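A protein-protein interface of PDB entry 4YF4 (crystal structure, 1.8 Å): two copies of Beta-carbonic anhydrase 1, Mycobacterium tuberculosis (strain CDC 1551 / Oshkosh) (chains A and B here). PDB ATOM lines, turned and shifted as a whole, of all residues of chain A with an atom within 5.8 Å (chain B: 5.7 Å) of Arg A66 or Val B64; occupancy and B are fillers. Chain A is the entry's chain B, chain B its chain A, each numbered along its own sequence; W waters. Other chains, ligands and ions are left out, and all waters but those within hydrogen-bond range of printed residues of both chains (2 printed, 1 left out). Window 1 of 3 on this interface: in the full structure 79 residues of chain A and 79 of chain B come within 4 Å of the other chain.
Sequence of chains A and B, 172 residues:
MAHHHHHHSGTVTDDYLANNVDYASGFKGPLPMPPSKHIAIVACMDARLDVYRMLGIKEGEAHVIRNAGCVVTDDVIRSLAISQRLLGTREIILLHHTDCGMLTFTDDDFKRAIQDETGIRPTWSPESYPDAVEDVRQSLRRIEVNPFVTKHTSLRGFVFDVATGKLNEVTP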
ATOM      1  N   ILE A  41      16.920  33.028  10.177  1.00  0.00           N
ATOM      2  CA  ILE A  41      18.122  33.636  10.740  1.00  0.00           C
ATOM      3  C   ILE A  41      19.095  32.505  11.029  1.00  0.00           C
ATOM      4  O   ILE A  41      18.719  31.502  11.629  1.00  0.00           O
ATOM      5  CB  ILE A  41      17.848  34.324  12.104  1.00  0.00           C
ATOM      6  CG1 ILE A  41      16.508  35.069  12.103  1.00  0.00           C
ATOM      7  CG2 ILE A  41      19.028  35.222  12.501  1.00  0.00           C
ATOM      8  CD1 ILE A  41      16.502  36.310  11.301  1.00  0.00           C
ATOM      9  N   VAL A  42      20.330  32.644  10.574  1.00  0.00           N
ATOM     10  CA  VAL A  42      21.363  31.704  10.966  1.00  0.00           C
ATOM     11  C   VAL A  42      22.231  32.455  11.951  1.00  0.00           C
ATOM     12  O   VAL A  42      22.735  33.526  11.630  1.00  0.00           O
ATOM     13  CB  VAL A  42      22.206  31.258   9.764  1.00  0.00           C
ATOM     14  CG1 VAL A  42      23.317  30.308  10.212  1.00  0.00           C
ATOM     15  CG2 VAL A  42      21.329  30.594   8.713  1.00  0.00           C
ATOM     16  N   ALA A  43      22.389  31.928  13.160  1.00  0.00           N
ATOM     17  CA  ALA A  43      23.106  32.672  14.175  1.00  0.00           C
ATOM     18  C   ALA A  43      24.046  31.775  14.987  1.00  0.00           C
ATOM     19  O   ALA A  43      24.173  30.586  14.725  1.00  0.00           O
ATOM     20  CB  ALA A  43      22.118  33.413  15.093  1.00  0.00           C
ATOM     21  N   CYS A  44      24.794  32.400  15.939  1.00  0.00           N
ATOM     22  CA  CYS A  44      25.737  31.683  16.785  1.00  0.00           C
ATOM     23  C   CYS A  44      25.040  31.176  18.028  1.00  0.00           C
ATOM     24  O   CYS A  44      24.073  31.778  18.481  1.00  0.00           O
ATOM     25  CB  CYS A  44      26.854  32.621  17.214  1.00  0.00           C
ATOM     26  SG  CYS A  44      28.169  31.808  18.061  1.00  0.00           S
ATOM     27  N   MET A  45      25.483  30.058  18.602  1.00  0.00           N
ATOM     28  CA  MET A  45      24.943  29.568  19.866  1.00  0.00           C
ATOM     29  C   MET A  45      25.392  30.431  21.035  1.00  0.00           C
ATOM     30  O   MET A  45      24.847  30.310  22.134  1.00  0.00           O
ATOM     31  CB  MET A  45      25.339  28.108  20.113  1.00  0.00           C
ATOM     32  CG  MET A  45      26.810  27.885  20.395  1.00  0.00           C
ATOM     33  SD  MET A  45      27.193  26.147  20.772  1.00  0.00           S
ATOM     34  CE  MET A  45      28.885  26.341  21.330  1.00  0.00           C
ATOM     35  N   ASP A  46      26.384  31.286  20.789  1.00  0.00           N
ATOM     36  CA  ASP A  46      26.968  32.164  21.807  1.00  0.00           C
ATOM     37  C   ASP A  46      25.969  32.725  22.821  1.00  0.00           C
ATOM     38  O   ASP A  46      24.895  33.223  22.466  1.00  0.00           O
ATOM     39  CB  ASP A  46      27.745  33.303  21.137  1.00  0.00           C
ATOM     40  CG  ASP A  46      28.628  34.064  22.112  1.00  0.00           C
ATOM     41  OD1 ASP A  46      28.132  35.015  22.764  1.00  0.00           O
ATOM     42  OD2 ASP A  46      29.820  33.705  22.230  1.00  0.00           O
ATOM     43  N   ALA A  47      26.324  32.611  24.095  1.00  0.00           N
ATOM     44  CA  ALA A  47      25.399  32.934  25.179  1.00  0.00           C
ATOM     45  C   ALA A  47      25.025  34.416  25.243  1.00  0.00           C
ATOM     46  O   ALA A  47      24.037  34.791  25.876  1.00  0.00           O
ATOM     47  CB  ALA A  47      25.964  32.458  26.525  1.00  0.00           C
ATOM     48  N   LEU A  49      24.128  36.257  22.789  1.00  0.00           N
ATOM     49  CA  LEU A  49      23.299  36.612  21.653  1.00  0.00           C
ATOM     50  C   LEU A  49      21.874  36.150  21.888  1.00  0.00           C
ATOM     51  O   LEU A  49      21.562  34.961  21.789  1.00  0.00           O
ATOM     52  CB  LEU A  49      23.845  36.008  20.350  1.00  0.00           C
ATOM     53  CG  LEU A  49      24.933  36.790  19.605  1.00  0.00           C
ATOM     54  CD1 LEU A  49      26.196  36.933  20.439  1.00  0.00           C
ATOM     55  CD2 LEU A  49      25.241  36.111  18.281  1.00  0.00           C
ATOM     56  N   ASP A  50      21.030  37.104  22.261  1.00  0.00           N
ATOM     57  CA  ASP A  50      19.603  36.874  22.380  1.00  0.00           C
ATOM     58  C   ASP A  50      19.043  37.356  21.048  1.00  0.00           C
ATOM     59  O   ASP A  50      18.634  38.512  20.915  1.00  0.00           O
ATOM     60  CB  ASP A  50      19.044  37.690  23.544  1.00  0.00           C
ATOM     61  CG  ASP A  50      17.570  37.436  23.797  1.00  0.00           C
ATOM     62  OD1 ASP A  50      16.921  36.702  23.023  1.00  0.00           O
ATOM     63  OD2 ASP A  50      17.059  37.993  24.787  1.00  0.00           O
ATOM     64  N   VAL A  51      19.056  36.459  20.066  1.00  0.00           N
ATOM     65  CA  VAL A  51      18.678  36.776  18.680  1.00  0.00           C
ATOM     66  C   VAL A  51      17.299  37.425  18.561  1.00  0.00           C
ATOM     67  O   VAL A  51      17.112  38.379  17.798  1.00  0.00           O
ATOM     68  CB  VAL A  51      18.695  35.513  17.802  1.00  0.00           C
ATOM     69  CG1 VAL A  51      18.178  35.832  16.389  1.00  0.00           C
ATOM     70  CG2 VAL A  51      20.117  34.907  17.762  1.00  0.00           C
ATOM     71  N   VAL A  64      14.818  30.455  13.410  1.00  0.00           N
ATOM     72  CA  VAL A  64      16.130  30.804  13.945  1.00  0.00           C
ATOM     73  C   VAL A  64      16.978  29.527  14.079  1.00  0.00           C
ATOM     74  O   VAL A  64      16.600  28.583  14.788  1.00  0.00           O
ATOM     75  CB  VAL A  64      16.008  31.509  15.320  1.00  0.00           C
ATOM     76  CG1 VAL A  64      17.399  31.811  15.907  1.00  0.00           C
ATOM     77  CG2 VAL A  64      15.165  32.788  15.195  1.00  0.00           C
ATOM     78  N   ILE A  65      18.104  29.501  13.375  1.00  0.00           N
ATOM     79  CA  ILE A  65      19.007  28.357  13.353  1.00  0.00           C
ATOM     80  C   ILE A  65      20.306  28.809  14.022  1.00  0.00           C
ATOM     81  O   ILE A  65      20.804  29.906  13.738  1.00  0.00           O
ATOM     82  CB  ILE A  65      19.324  27.956  11.884  1.00  0.00           C
ATOM     83  CG1 ILE A  65      18.056  27.447  11.180  1.00  0.00           C
ATOM     84  CG2 ILE A  65      20.425  26.902  11.837  1.00  0.00           C
ATOM     85  CD1 ILE A  65      18.024  27.724   9.644  1.00  0.00           C
ATOM     86  N   ARG A  66      20.859  27.988  14.916  1.00  0.00           N
ATOM     87  CA  ARG A  66      22.057  28.386  15.645  1.00  0.00           C
ATOM     88  C   ARG A  66      22.973  27.189  15.834  1.00  0.00           C
ATOM     89  O   ARG A  66      22.516  26.099  16.179  1.00  0.00           O
ATOM     90  CB  ARG A  66      21.700  28.967  17.027  1.00  0.00           C
ATOM     91  CG  ARG A  66      20.692  30.122  16.995  1.00  0.00           C
ATOM     92  CD  ARG A  66      20.307  30.587  18.396  1.00  0.00           C
ATOM     93  NE  ARG A  66      21.409  31.298  19.032  1.00  0.00           N
ATOM     94  CZ  ARG A  66      21.269  32.156  20.036  1.00  0.00           C
ATOM     95  NH1 ARG A  66      20.067  32.439  20.519  1.00  0.00           N
ATOM     96  NH2 ARG A  66      22.341  32.739  20.545  1.00  0.00           N
ATOM     97  N   ASN A  67      24.259  27.392  15.576  1.00  0.00           N
ATOM     98  CA  ASN A  67      25.287  26.426  15.937  1.00  0.00           C
ATOM     99  C   ASN A  67      26.556  27.114  16.461  1.00  0.00           C
ATOM    100  O   ASN A  67      26.589  28.335  16.614  1.00  0.00           O
ATOM    101  CB  ASN A  67      25.595  25.508  14.750  1.00  0.00           C
ATOM    102  CG  ASN A  67      26.244  26.251  13.592  1.00  0.00           C
ATOM    103  OD1 ASN A  67      26.754  27.355  13.757  1.00  0.00           O
ATOM    104  ND2 ASN A  67      26.229  25.637  12.415  1.00  0.00           N
ATOM    105  N   ALA A  68      27.606  26.334  16.714  1.00  0.00           N
ATOM    106  CA  ALA A  68      28.878  26.905  17.146  1.00  0.00           C
ATOM    107  C   ALA A  68      29.529  27.685  16.009  1.00  0.00           C
ATOM    108  O   ALA A  68      29.917  27.108  14.988  1.00  0.00           O
ATOM    109  CB  ALA A  68      29.810  25.813  17.639  1.00  0.00           C
ATOM    110  N   ALA B  40      23.605  24.087  27.959  1.00  0.00           N
ATOM    111  CA  ALA B  40      23.326  24.157  26.526  1.00  0.00           C
ATOM    112  C   ALA B  40      21.912  23.659  26.226  1.00  0.00           C
ATOM    113  O   ALA B  40      21.479  22.624  26.749  1.00  0.00           O
ATOM    114  CB  ALA B  40      24.360  23.347  25.744  1.00  0.00           C
ATOM    115  N   ILE B  41      21.190  24.417  25.402  1.00  0.00           N
ATOM    116  CA  ILE B  41      19.860  24.041  24.946  1.00  0.00           C
ATOM    117  C   ILE B  41      19.973  23.626  23.480  1.00  0.00           C
ATOM    118  O   ILE B  41      20.573  24.346  22.683  1.00  0.00           O
ATOM    119  CB  ILE B  41      18.892  25.252  25.008  1.00  0.00           C
ATOM    120  CG1 ILE B  41      19.180  26.138  26.230  1.00  0.00           C
ATOM    121  CG2 ILE B  41      17.422  24.798  24.933  1.00  0.00           C
ATOM    122  CD1 ILE B  41      18.692  25.576  27.536  1.00  0.00           C
ATOM    123  N   ALA B  43      17.426  22.994  20.442  1.00  0.00           N
ATOM    124  CA  ALA B  43      16.035  23.257  20.175  1.00  0.00           C
ATOM    125  C   ALA B  43      15.734  23.250  18.681  1.00  0.00           C
ATOM    126  O   ALA B  43      16.623  23.100  17.838  1.00  0.00           O
ATOM    127  CB  ALA B  43      15.620  24.590  20.794  1.00  0.00           C
ATOM    128  N   VAL B  51      12.956  30.383  22.590  1.00  0.00           N
ATOM    129  CA  VAL B  51      13.685  29.602  23.597  1.00  0.00           C
ATOM    130  C   VAL B  51      14.043  30.391  24.864  1.00  0.00           C
ATOM    131  O   VAL B  51      13.833  29.912  25.980  1.00  0.00           O
ATOM    132  CB  VAL B  51      14.943  28.948  22.994  1.00  0.00           C
ATOM    133  CG1 VAL B  51      15.728  28.213  24.053  1.00  0.00           C
ATOM    134  CG2 VAL B  51      14.544  27.983  21.873  1.00  0.00           C
ATOM    135  N   TYR B  52      14.558  31.604  24.692  1.00  0.00           N
ATOM    136  CA  TYR B  52      14.908  32.443  25.838  1.00  0.00           C
ATOM    137  C   TYR B  52      13.709  32.704  26.767  1.00  0.00           C
ATOM    138  O   TYR B  52      13.797  32.507  27.986  1.00  0.00           O
ATOM    139  CB  TYR B  52      15.509  33.775  25.363  1.00  0.00           C
ATOM    140  CG  TYR B  52      17.030  33.812  25.235  1.00  0.00           C
ATOM    141  CD1 TYR B  52      17.704  32.994  24.329  1.00  0.00           C
ATOM    142  CD2 TYR B  52      17.787  34.696  26.007  1.00  0.00           C
ATOM    143  CE1 TYR B  52      19.105  33.054  24.207  1.00  0.00           C
ATOM    144  CE2 TYR B  52      19.183  34.759  25.898  1.00  0.00           C
ATOM    145  CZ  TYR B  52      19.830  33.941  24.999  1.00  0.00           C
ATOM    146  OH  TYR B  52      21.204  34.025  24.897  1.00  0.00           O
ATOM    147  N   ILE B  57      15.565  32.539  30.257  1.00  0.00           N
ATOM    148  CA  ILE B  57      17.008  32.721  30.093  1.00  0.00           C
ATOM    149  C   ILE B  57      17.376  34.202  29.966  1.00  0.00           C
ATOM    150  O   ILE B  57      16.668  34.962  29.307  1.00  0.00           O
ATOM    151  CB  ILE B  57      17.518  32.000  28.826  1.00  0.00           C
ATOM    152  CG1 ILE B  57      17.061  30.535  28.804  1.00  0.00           C
ATOM    153  CG2 ILE B  57      19.049  32.102  28.709  1.00  0.00           C
ATOM    154  CD1 ILE B  57      17.439  29.792  27.530  1.00  0.00           C
ATOM    155  N   ALA B  62      23.427  30.935  28.693  1.00  0.00           N
ATOM    156  CA  ALA B  62      23.190  29.632  28.072  1.00  0.00           C
ATOM    157  C   ALA B  62      23.558  29.610  26.594  1.00  0.00           C
ATOM    158  O   ALA B  62      23.282  30.564  25.874  1.00  0.00           O
ATOM    159  CB  ALA B  62      21.698  29.268  28.215  1.00  0.00           C
ATOM    160  N   HIS B  63      24.174  28.525  26.141  1.00  0.00           N
ATOM    161  CA  HIS B  63      24.293  28.310  24.709  1.00  0.00           C
ATOM    162  C   HIS B  63      22.952  27.818  24.215  1.00  0.00           C
ATOM    163  O   HIS B  63      22.292  27.005  24.881  1.00  0.00           O
ATOM    164  CB  HIS B  63      25.355  27.268  24.385  1.00  0.00           C
ATOM    165  CG  HIS B  63      26.751  27.789  24.449  1.00  0.00           C
ATOM    166  ND1 HIS B  63      27.822  26.995  24.796  1.00  0.00           N
ATOM    167  CD2 HIS B  63      27.257  29.025  24.211  1.00  0.00           C
ATOM    168  CE1 HIS B  63      28.926  27.721  24.782  1.00  0.00           C
ATOM    169  NE2 HIS B  63      28.612  28.954  24.423  1.00  0.00           N
ATOM    170  N   VAL B  64      22.541  28.309  23.053  1.00  0.00           N
ATOM    171  CA  VAL B  64      21.331  27.821  22.407  1.00  0.00           C
ATOM    172  C   VAL B  64      21.642  27.343  20.988  1.00  0.00           C
ATOM    173  O   VAL B  64      22.135  28.118  20.159  1.00  0.00           O
ATOM    174  CB  VAL B  64      20.228  28.915  22.398  1.00  0.00           C
ATOM    175  CG1 VAL B  64      18.980  28.423  21.704  1.00  0.00           C
ATOM    176  CG2 VAL B  64      19.896  29.356  23.835  1.00  0.00           C
ATOM    177  N   ILE B  65      21.367  26.069  20.717  1.00  0.00           N
ATOM    178  CA  ILE B  65      21.648  25.452  19.422  1.00  0.00           C
ATOM    179  C   ILE B  65      20.286  25.114  18.817  1.00  0.00           C
ATOM    180  O   ILE B  65      19.417  24.584  19.523  1.00  0.00           O
ATOM    181  CB  ILE B  65      22.485  24.161  19.600  1.00  0.00           C
ATOM    182  CG1 ILE B  65      23.844  24.504  20.213  1.00  0.00           C
ATOM    183  CG2 ILE B  65      22.683  23.439  18.263  1.00  0.00           C
ATOM    184  CD1 ILE B  65      24.472  23.357  20.945  1.00  0.00           C
ATOM    185  N   ARG B  66      20.061  25.486  17.551  1.00  0.00           N
ATOM    186  CA  ARG B  66      18.760  25.250  16.919  1.00  0.00           C
ATOM    187  C   ARG B  66      18.915  24.805  15.476  1.00  0.00           C
ATOM    188  O   ARG B  66      19.733  25.358  14.736  1.00  0.00           O
ATOM    189  CB  ARG B  66      17.871  26.507  16.972  1.00  0.00           C
ATOM    190  CG  ARG B  66      17.716  27.109  18.376  1.00  0.00           C
ATOM    191  CD  ARG B  66      16.896  28.390  18.364  1.00  0.00           C
ATOM    192  NE  ARG B  66      15.520  28.109  17.990  1.00  0.00           N
ATOM    193  CZ  ARG B  66      14.498  28.915  18.247  1.00  0.00           C
ATOM    194  NH1 ARG B  66      14.695  30.060  18.898  1.00  0.00           N
ATOM    195  NH2 ARG B  66      13.278  28.563  17.867  1.00  0.00           N
ATOM    196  N   ASN B  67      18.134  23.801  15.081  1.00  0.00           N
ATOM    197  CA  ASN B  67      18.065  23.409  13.676  1.00  0.00           C
ATOM    198  C   ASN B  67      16.667  22.892  13.313  1.00  0.00           C
ATOM    199  O   ASN B  67      15.768  22.866  14.168  1.00  0.00           O
ATOM    200  CB  ASN B  67      19.156  22.375  13.363  1.00  0.00           C
ATOM    201  CG  ASN B  67      18.909  21.027  14.072  1.00  0.00           C
ATOM    202  OD1 ASN B  67      17.844  20.795  14.658  1.00  0.00           O
ATOM    203  ND2 ASN B  67      19.879  20.138  13.984  1.00  0.00           N
ATOM    204  N   SER B  79      28.778  21.258  18.056  1.00  0.00           N
ATOM    205  CA  SER B  79      28.493  22.445  18.855  1.00  0.00           C
ATOM    206  C   SER B  79      28.489  22.116  20.354  1.00  0.00           C
ATOM    207  O   SER B  79      29.008  22.882  21.165  1.00  0.00           O
ATOM    208  CB  SER B  79      27.198  23.139  18.415  1.00  0.00           C
ATOM    209  OG  SER B  79      27.257  23.436  17.024  1.00  0.00           O
HETATM  210  O   HOH W   1      29.197  31.930  24.530  1.00  0.00           O
HETATM  211  O   HOH W   2      21.997  33.155  27.495  1.00  0.00           O
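OH of Tyr B52 sits at hydrogen-bond distance from O of Ala A47, 3.1 Å away. The backbone carbonyl oxygen (O) of Leu A49 is in hydrogen-bond range of the side-chain hydroxyl (OH) of Tyr B52. O of Met A45 sits at hydrogen-bond distance from N of Val B64. O of Val B64 lies close to NE of Arg A66 (3.5 Å). The backbone carbonyl oxygen (O) of Val A64 lies close to the guanidinium group (NE) of Arg B66 (3.4 Å). The backbone NH (N) of Arg A66 is in hydrogen-bond range of the backbone carbonyl oxygen (O) of Arg B66 (2.9 Å). N of Ala A68 sits at hydrogen-bond distance from OG of Ser B79, 2.9 Å away. SD of Met A45 sits close to O of Ser B79.
Of the 15 printed residues of chain A, 10 touch a printed residue of chain B. Hydrophobic or aromatic side chains of chain A that line the printed part of chain B: Met A45, Ala A47, Ile A65 and Ala A68. Of the 13 printed residues of chain B, 7 touch a printed residue of chain A. Hydrophobic or aromatic side chains of chain B within 4 Å of the printed part of chain A: Tyr B52, His B63, Val B64 and Ile B65. Among the printed residues, 18 pairs touch across the chains.
Water W2 lies within hydrogen-bond range of OH of Tyr B52, N of Ala B62 and O of Ala A47. Water W1 lies within hydrogen-bond range of OD2 of Asp A46, N of Ala A47 and NE2 of His B63.
CA of His B63 touches O of Met A45 (3.3 Å). Ile B65 touches Met A45 (CG1 to SD, 3.8 Å). Asp A46 touches His B63 (CA to CD2, 3.96 Å). CA of Ala A47 touches O of Ala B62, at 3.3 Å. Ala A47 touches His B63. Tyr B52 touches Asp A50 (CD2 to CG, 3.5 Å). Ile A65 touches Arg B66. Arg A66 touches Tyr B52 (NH1 to CE1, 3.9 Å). Arg A66 touches Ile B65. Ser B79 touches Asn A67 (OG to CB, 3.5 Å).
N of Ile B41 is in hydrogen-bond range of O of His B63 (2.9 Å). The backbone NH (N) of Ala B43 sits at hydrogen-bond distance from the backbone carbonyl oxygen (O) of Ile B65 (2.7 Å). The backbone carbonyl oxygen of Ile A41 is in hydrogen-bond range of the backbone NH of Ile A65 (2.7 Å). N of Ala A43 sits at hydrogen-bond distance from O of Ile A65. N of Met A45 lies within hydrogen-bond range of O of Asn A67, 2.9 Å away. NH2 of Arg A66 is in hydrogen-bond range of O of Asp A46, 3.2 Å away.
Val A51 touches none of the printed residues of chain B. Of chain B, only Tyr B52 (3.9 Å), Val B64 (3.3 Å), Ile B65 (3.4 Å) and Arg B66 (2.9 Å) come within 4 Å of Arg A66. Printed residues of chain A within 4 Å of Tyr B52: Ala A47, Leu A49, Asp A50 and Arg A66. Ile B57 touches none of the printed residues of chain A. Of the printed residues of chain A, His B63 touches Met A45, Asp A46 and Ala A47. The nearest residue of chain B that does not touch Arg A66 is Asn B67 (5.0 Å). The nearest printed residue of chain A that does not touch Val B64 is Cys A44 (4.5 Å). The nearest printed residue of chain A that does not touch Ile B65 is Asn A67 (4.6 Å).
Val A64 touches Arg B66, and with the chains exchanged Arg A66 touches Val B64. Ile A65 touches Arg B66, and with the chains exchanged Arg A66 touches Ile B65. Arg A66 touches its own counterpart, Arg B66.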
